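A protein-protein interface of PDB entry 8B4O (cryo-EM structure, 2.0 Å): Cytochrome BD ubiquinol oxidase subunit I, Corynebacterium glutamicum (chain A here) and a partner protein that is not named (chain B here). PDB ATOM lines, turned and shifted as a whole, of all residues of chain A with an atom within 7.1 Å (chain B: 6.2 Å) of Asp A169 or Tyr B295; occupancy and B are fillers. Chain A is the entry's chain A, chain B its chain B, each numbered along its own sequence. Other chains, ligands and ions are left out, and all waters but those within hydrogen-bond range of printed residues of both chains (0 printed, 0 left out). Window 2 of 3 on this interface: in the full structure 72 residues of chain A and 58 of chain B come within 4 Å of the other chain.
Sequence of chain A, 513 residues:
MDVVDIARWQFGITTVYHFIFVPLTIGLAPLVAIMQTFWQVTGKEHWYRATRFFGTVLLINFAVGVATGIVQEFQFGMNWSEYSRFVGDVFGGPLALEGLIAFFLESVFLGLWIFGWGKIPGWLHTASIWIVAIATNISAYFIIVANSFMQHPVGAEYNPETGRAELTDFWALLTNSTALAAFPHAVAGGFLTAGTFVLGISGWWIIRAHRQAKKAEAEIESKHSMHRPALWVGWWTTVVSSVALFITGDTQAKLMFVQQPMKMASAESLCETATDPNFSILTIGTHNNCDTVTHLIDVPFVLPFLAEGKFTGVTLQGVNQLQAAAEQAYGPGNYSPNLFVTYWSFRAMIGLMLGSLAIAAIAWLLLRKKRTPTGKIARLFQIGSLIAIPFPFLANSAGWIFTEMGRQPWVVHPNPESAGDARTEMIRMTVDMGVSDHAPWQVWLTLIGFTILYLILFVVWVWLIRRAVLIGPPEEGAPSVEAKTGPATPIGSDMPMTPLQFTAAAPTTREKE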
ATOM      1  N   ASP A  89      30.086   8.109  -0.519  1.00  0.00           N
ATOM      2  CA  ASP A  89      28.987   7.677   0.338  1.00  0.00           C
ATOM      3  C   ASP A  89      28.899   8.530   1.596  1.00  0.00           C
ATOM      4  O   ASP A  89      27.810   8.963   1.990  1.00  0.00           O
ATOM      5  CB  ASP A  89      29.175   6.203   0.700  1.00  0.00           C
ATOM      6  CG  ASP A  89      27.979   5.617   1.419  1.00  0.00           C
ATOM      7  OD1 ASP A  89      27.705   6.024   2.566  1.00  0.00           O
ATOM      8  OD2 ASP A  89      27.306   4.749   0.832  1.00  0.00           O
ATOM      9  N   VAL A  90      30.038   8.797   2.224  1.00  0.00           N
ATOM     10  CA  VAL A  90      30.111   9.462   3.518  1.00  0.00           C
ATOM     11  C   VAL A  90      30.620  10.894   3.387  1.00  0.00           C
ATOM     12  O   VAL A  90      30.182  11.789   4.113  1.00  0.00           O
ATOM     13  CB  VAL A  90      30.979   8.651   4.506  1.00  0.00           C
ATOM     14  CG1 VAL A  90      32.397   8.590   4.020  1.00  0.00           C
ATOM     15  CG2 VAL A  90      30.944   9.272   5.887  1.00  0.00           C
ATOM     16  N   VAL A 154      35.586   9.129  10.745  1.00  0.00           N
ATOM     17  CA  VAL A 154      34.692   8.608  11.770  1.00  0.00           C
ATOM     18  C   VAL A 154      33.297   8.482  11.177  1.00  0.00           C
ATOM     19  O   VAL A 154      32.961   9.122  10.179  1.00  0.00           O
ATOM     20  CB  VAL A 154      34.649   9.499  13.029  1.00  0.00           C
ATOM     21  CG1 VAL A 154      35.979   9.478  13.740  1.00  0.00           C
ATOM     22  CG2 VAL A 154      34.264  10.917  12.654  1.00  0.00           C
ATOM     23  N   GLY A 155      32.478   7.652  11.815  1.00  0.00           N
ATOM     24  CA  GLY A 155      31.125   7.445  11.345  1.00  0.00           C
ATOM     25  C   GLY A 155      31.027   6.684  10.046  1.00  0.00           C
ATOM     26  O   GLY A 155      30.027   6.814   9.337  1.00  0.00           O
ATOM     27  N   ALA A 156      32.041   5.898   9.707  1.00  0.00           N
ATOM     28  CA  ALA A 156      32.066   5.167   8.453  1.00  0.00           C
ATOM     29  C   ALA A 156      32.511   3.736   8.708  1.00  0.00           C
ATOM     30  O   ALA A 156      33.306   3.466   9.610  1.00  0.00           O
ATOM     31  CB  ALA A 156      32.998   5.835   7.434  1.00  0.00           C
ATOM     32  N   GLU A 157      31.984   2.818   7.904  1.00  0.00           N
ATOM     33  CA  GLU A 157      32.375   1.417   7.957  1.00  0.00           C
ATOM     34  C   GLU A 157      32.704   0.941   6.553  1.00  0.00           C
ATOM     35  O   GLU A 157      31.996   1.279   5.599  1.00  0.00           O
ATOM     36  CB  GLU A 157      31.273   0.551   8.563  1.00  0.00           C
ATOM     37  CG  GLU A 157      31.358   0.430  10.071  1.00  0.00           C
ATOM     38  CD  GLU A 157      30.132  -0.216  10.656  1.00  0.00           C
ATOM     39  OE1 GLU A 157      29.657   0.234  11.721  1.00  0.00           O
ATOM     40  OE2 GLU A 157      29.643  -1.184  10.042  1.00  0.00           O
ATOM     41  N   GLU A 166      31.445   3.437   3.851  1.00  0.00           N
ATOM     42  CA  GLU A 166      30.031   3.773   3.794  1.00  0.00           C
ATOM     43  C   GLU A 166      29.568   4.412   5.095  1.00  0.00           C
ATOM     44  O   GLU A 166      30.045   4.060   6.178  1.00  0.00           O
ATOM     45  CB  GLU A 166      29.195   2.531   3.485  1.00  0.00           C
ATOM     46  CG  GLU A 166      29.569   1.868   2.168  1.00  0.00           C
ATOM     47  CD  GLU A 166      28.712   0.665   1.849  1.00  0.00           C
ATOM     48  OE1 GLU A 166      28.575   0.336   0.653  1.00  0.00           O
ATOM     49  OE2 GLU A 166      28.174   0.047   2.790  1.00  0.00           O
ATOM     50  N   LEU A 167      28.633   5.351   4.975  1.00  0.00           N
ATOM     51  CA  LEU A 167      28.132   6.084   6.130  1.00  0.00           C
ATOM     52  C   LEU A 167      27.324   5.169   7.041  1.00  0.00           C
ATOM     53  O   LEU A 167      26.462   4.415   6.582  1.00  0.00           O
ATOM     54  CB  LEU A 167      27.275   7.261   5.666  1.00  0.00           C
ATOM     55  CG  LEU A 167      26.703   8.204   6.725  1.00  0.00           C
ATOM     56  CD1 LEU A 167      27.798   8.959   7.454  1.00  0.00           C
ATOM     57  CD2 LEU A 167      25.711   9.167   6.101  1.00  0.00           C
ATOM     58  N   THR A 168      27.609   5.237   8.338  1.00  0.00           N
ATOM     59  CA  THR A 168      26.906   4.443   9.334  1.00  0.00           C
ATOM     60  C   THR A 168      26.513   5.227  10.575  1.00  0.00           C
ATOM     61  O   THR A 168      25.734   4.720  11.382  1.00  0.00           O
ATOM     62  CB  THR A 168      27.755   3.239   9.766  1.00  0.00           C
ATOM     63  OG1 THR A 168      27.008   2.434  10.682  1.00  0.00           O
ATOM     64  CG2 THR A 168      29.023   3.706  10.447  1.00  0.00           C
ATOM     65  N   ASP A 169      27.037   6.438  10.756  1.00  0.00           N
ATOM     66  CA  ASP A 169      26.687   7.284  11.895  1.00  0.00           C
ATOM     67  C   ASP A 169      26.843   8.738  11.471  1.00  0.00           C
ATOM     68  O   ASP A 169      27.960   9.262  11.438  1.00  0.00           O
ATOM     69  CB  ASP A 169      27.558   6.967  13.109  1.00  0.00           C
ATOM     70  CG  ASP A 169      27.054   7.628  14.373  1.00  0.00           C
ATOM     71  OD1 ASP A 169      25.935   8.181  14.354  1.00  0.00           O
ATOM     72  OD2 ASP A 169      27.775   7.589  15.389  1.00  0.00           O
ATOM     73  N   PHE A 170      25.723   9.384  11.148  1.00  0.00           N
ATOM     74  CA  PHE A 170      25.760  10.770  10.691  1.00  0.00           C
ATOM     75  C   PHE A 170      26.233  11.711  11.792  1.00  0.00           C
ATOM     76  O   PHE A 170      26.985  12.658  11.529  1.00  0.00           O
ATOM     77  CB  PHE A 170      24.379  11.177  10.193  1.00  0.00           C
ATOM     78  CG  PHE A 170      24.358  12.478   9.460  1.00  0.00           C
ATOM     79  CD1 PHE A 170      25.305  12.757   8.491  1.00  0.00           C
ATOM     80  CD2 PHE A 170      23.373  13.413   9.719  1.00  0.00           C
ATOM     81  CE1 PHE A 170      25.279  13.949   7.807  1.00  0.00           C
ATOM     82  CE2 PHE A 170      23.341  14.605   9.035  1.00  0.00           C
ATOM     83  CZ  PHE A 170      24.296  14.872   8.078  1.00  0.00           C
ATOM     84  N   TRP A 171      25.788  11.474  13.028  1.00  0.00           N
ATOM     85  CA  TRP A 171      26.142  12.362  14.129  1.00  0.00           C
ATOM     86  C   TRP A 171      27.636  12.322  14.411  1.00  0.00           C
ATOM     87  O   TRP A 171      28.243  13.353  14.718  1.00  0.00           O
ATOM     88  CB  TRP A 171      25.343  11.990  15.378  1.00  0.00           C
ATOM     89  CG  TRP A 171      25.455  12.991  16.482  1.00  0.00           C
ATOM     90  CD1 TRP A 171      26.122  12.841  17.661  1.00  0.00           C
ATOM     91  CD2 TRP A 171      24.893  14.308  16.504  1.00  0.00           C
ATOM     92  NE1 TRP A 171      26.005  13.980  18.418  1.00  0.00           N
ATOM     93  CE2 TRP A 171      25.256  14.896  17.729  1.00  0.00           C
ATOM     94  CE3 TRP A 171      24.120  15.047  15.604  1.00  0.00           C
ATOM     95  CZ2 TRP A 171      24.870  16.187  18.080  1.00  0.00           C
ATOM     96  CZ3 TRP A 171      23.737  16.328  15.953  1.00  0.00           C
ATOM     97  CH2 TRP A 171      24.112  16.884  17.181  1.00  0.00           C
ATOM     98  N   ALA A 172      28.246  11.140  14.316  1.00  0.00           N
ATOM     99  CA  ALA A 172      29.685  11.037  14.526  1.00  0.00           C
ATOM    100  C   ALA A 172      30.450  11.803  13.460  1.00  0.00           C
ATOM    101  O   ALA A 172      31.507  12.380  13.737  1.00  0.00           O
ATOM    102  CB  ALA A 172      30.114   9.573  14.544  1.00  0.00           C
ATOM    103  N   LEU A 173      29.943  11.804  12.226  1.00  0.00           N
ATOM    104  CA  LEU A 173      30.578  12.570  11.162  1.00  0.00           C
ATOM    105  C   LEU A 173      30.459  14.066  11.424  1.00  0.00           C
ATOM    106  O   LEU A 173      31.456  14.795  11.378  1.00  0.00           O
ATOM    107  CB  LEU A 173      29.955  12.206   9.815  1.00  0.00           C
ATOM    108  CG  LEU A 173      30.461  12.950   8.575  1.00  0.00           C
ATOM    109  CD1 LEU A 173      31.826  12.437   8.163  1.00  0.00           C
ATOM    110  CD2 LEU A 173      29.478  12.833   7.431  1.00  0.00           C
ATOM    111  N   LEU A 174      29.244  14.540  11.712  1.00  0.00           N
ATOM    112  CA  LEU A 174      29.037  15.971  11.913  1.00  0.00           C
ATOM    113  C   LEU A 174      29.807  16.488  13.122  1.00  0.00           C
ATOM    114  O   LEU A 174      30.402  17.570  13.072  1.00  0.00           O
ATOM    115  CB  LEU A 174      27.550  16.283  12.065  1.00  0.00           C
ATOM    116  CG  LEU A 174      26.695  16.237  10.805  1.00  0.00           C
ATOM    117  CD1 LEU A 174      25.294  16.706  11.124  1.00  0.00           C
ATOM    118  CD2 LEU A 174      27.310  17.087   9.714  1.00  0.00           C
ATOM    119  N   SER B 293      24.930   4.009   0.126  1.00  0.00           N
ATOM    120  CA  SER B 293      24.335   3.067   1.057  1.00  0.00           C
ATOM    121  C   SER B 293      22.904   3.468   1.380  1.00  0.00           C
ATOM    122  O   SER B 293      22.461   4.581   1.091  1.00  0.00           O
ATOM    123  CB  SER B 293      25.144   3.004   2.347  1.00  0.00           C
ATOM    124  OG  SER B 293      26.435   2.504   2.089  1.00  0.00           O
ATOM    125  N   HIS B 294      22.172   2.537   1.994  1.00  0.00           N
ATOM    126  CA  HIS B 294      20.821   2.859   2.435  1.00  0.00           C
ATOM    127  C   HIS B 294      20.841   3.905   3.541  1.00  0.00           C
ATOM    128  O   HIS B 294      20.018   4.828   3.547  1.00  0.00           O
ATOM    129  CB  HIS B 294      20.098   1.597   2.900  1.00  0.00           C
ATOM    130  CG  HIS B 294      18.722   1.858   3.421  1.00  0.00           C
ATOM    131  ND1 HIS B 294      17.616   1.920   2.601  1.00  0.00           N
ATOM    132  CD2 HIS B 294      18.272   2.088   4.677  1.00  0.00           C
ATOM    133  CE1 HIS B 294      16.544   2.173   3.329  1.00  0.00           C
ATOM    134  NE2 HIS B 294      16.915   2.279   4.592  1.00  0.00           N
ATOM    135  N   TYR B 295      21.775   3.780   4.483  1.00  0.00           N
ATOM    136  CA  TYR B 295      21.862   4.743   5.575  1.00  0.00           C
ATOM    137  C   TYR B 295      22.196   6.134   5.053  1.00  0.00           C
ATOM    138  O   TYR B 295      21.599   7.131   5.478  1.00  0.00           O
ATOM    139  CB  TYR B 295      22.904   4.283   6.592  1.00  0.00           C
ATOM    140  CG  TYR B 295      23.022   5.189   7.794  1.00  0.00           C
ATOM    141  CD1 TYR B 295      22.152   5.063   8.868  1.00  0.00           C
ATOM    142  CD2 TYR B 295      24.005   6.168   7.857  1.00  0.00           C
ATOM    143  CE1 TYR B 295      22.256   5.887   9.967  1.00  0.00           C
ATOM    144  CE2 TYR B 295      24.115   6.996   8.953  1.00  0.00           C
ATOM    145  CZ  TYR B 295      23.239   6.850  10.004  1.00  0.00           C
ATOM    146  OH  TYR B 295      23.342   7.672  11.099  1.00  0.00           O
ATOM    147  N   ALA B 296      23.154   6.220   4.129  1.00  0.00           N
ATOM    148  CA  ALA B 296      23.499   7.505   3.535  1.00  0.00           C
ATOM    149  C   ALA B 296      22.315   8.091   2.783  1.00  0.00           C
ATOM    150  O   ALA B 296      22.028   9.288   2.888  1.00  0.00           O
ATOM    151  CB  ALA B 296      24.703   7.347   2.609  1.00  0.00           C
ATOM    152  N   LEU B 297      21.605   7.255   2.025  1.00  0.00           N
ATOM    153  CA  LEU B 297      20.422   7.731   1.321  1.00  0.00           C
ATOM    154  C   LEU B 297      19.324   8.143   2.294  1.00  0.00           C
ATOM    155  O   LEU B 297      18.579   9.088   2.027  1.00  0.00           O
ATOM    156  CB  LEU B 297      19.922   6.665   0.349  1.00  0.00           C
ATOM    157  CG  LEU B 297      20.827   6.408  -0.860  1.00  0.00           C
ATOM    158  CD1 LEU B 297      20.246   5.336  -1.759  1.00  0.00           C
ATOM    159  CD2 LEU B 297      21.079   7.688  -1.640  1.00  0.00           C
ATOM    160  N   THR B 298      19.220   7.464   3.439  1.00  0.00           N
ATOM    161  CA  THR B 298      18.235   7.851   4.449  1.00  0.00           C
ATOM    162  C   THR B 298      18.552   9.222   5.040  1.00  0.00           C
ATOM    163  O   THR B 298      17.673  10.089   5.146  1.00  0.00           O
ATOM    164  CB  THR B 298      18.172   6.791   5.550  1.00  0.00           C
ATOM    165  OG1 THR B 298      17.528   5.616   5.045  1.00  0.00           O
ATOM    166  CG2 THR B 298      17.412   7.306   6.757  1.00  0.00           C
ATOM    167  N   ILE B 299      19.808   9.431   5.438  1.00  0.00           N
ATOM    168  CA  ILE B 299      20.220  10.724   5.979  1.00  0.00           C
ATOM    169  C   ILE B 299      20.005  11.823   4.947  1.00  0.00           C
ATOM    170  O   ILE B 299      19.486  12.904   5.260  1.00  0.00           O
ATOM    171  CB  ILE B 299      21.687  10.659   6.438  1.00  0.00           C
ATOM    172  CG1 ILE B 299      21.828   9.748   7.660  1.00  0.00           C
ATOM    173  CG2 ILE B 299      22.227  12.046   6.704  1.00  0.00           C
ATOM    174  CD1 ILE B 299      20.964  10.150   8.828  1.00  0.00           C
ATOM    175  N   LEU B 300      20.401  11.558   3.701  1.00  0.00           N
ATOM    176  CA  LEU B 300      20.216  12.535   2.638  1.00  0.00           C
ATOM    177  C   LEU B 300      18.744  12.830   2.409  1.00  0.00           C
ATOM    178  O   LEU B 300      18.368  13.978   2.177  1.00  0.00           O
ATOM    179  CB  LEU B 300      20.867  12.034   1.353  1.00  0.00           C
ATOM    180  CG  LEU B 300      22.389  12.040   1.270  1.00  0.00           C
ATOM    181  CD1 LEU B 300      22.821  11.269   0.040  1.00  0.00           C
ATOM    182  CD2 LEU B 300      22.915  13.461   1.237  1.00  0.00           C
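The side-chain hydroxyl (OG) of Ser B293 lies close to the side-chain carboxylate (OE2) of Glu A166, at 3.1 Å. The side-chain carboxylate (OD2) of Asp A89 is in hydrogen-bond range of the backbone NH (N) of Ser B293 (2.6 Å). N of Phe A170 is in hydrogen-bond range of OH of Tyr B295, at 2.9 Å.
The backbone carbonyl oxygen of Glu A157 lies within hydrogen-bond range of the backbone NH of Glu A166 (2.8 Å). The backbone NH of Thr A168 is in hydrogen-bond range of the backbone carbonyl oxygen of Gly A155. N of Asp A169 is in hydrogen-bond range of O of Gly A155, at 3.3 Å. The side-chain carboxylate (OD1) of Asp A89 sits at hydrogen-bond distance from the backbone NH (N) of Leu A167, at 2.7 Å.
Of chain B, only Tyr B295 comes within 4 Å of Asp A169. Tyr B295 touches four residues of chain A. Of the printed residues of chain B, Asp A89 touches Ser B293 and Ala B296. Of the printed residues of chain A, Ile B299 touches Phe A170 (3.5 Å). Of the printed residues of chain B, Thr A168 touches Tyr B295 (3.4 Å). Leu B297 touches none of the printed residues of chain A. The nearest residue of chain A that does not touch Tyr B295 is Trp A171 (4.9 Å). The nearest printed residue of chain B that does not touch Thr A168 is Ala B296 (6.2 Å).
Hydrophobic or aromatic side chains of chain B that line the printed part of chain A: Tyr B295, Ala B296 and Ile B299. Of the 15 printed residues of chain A, 6 touch a printed residue of chain B. Printed residues of chain A that touch a printed residue of chain B: Asp A89, Glu A166, Leu A167, Thr A168, Asp A169 and Phe A170. Hydrophobic or aromatic side chains of chain A that line the printed part of chain B: Leu A167 and Phe A170. Among the printed residues, no Asp or Glu carboxylate lies within 4 Å of a Lys or Arg side-chain nitrogen of the other chain.
Among the printed residues, pairs that only touch across the chains: Asp A89 with Ala B296 (3.3 Å), Leu A167 with Tyr B295 (3.3 Å), Leu A167 with Ala B296 (3.8 Å), Thr A168 with Tyr B295 (3.4 Å), Asp A169 with Tyr B295 (3.5 Å) and Phe A170 with Ile B299 (3.5 Å).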
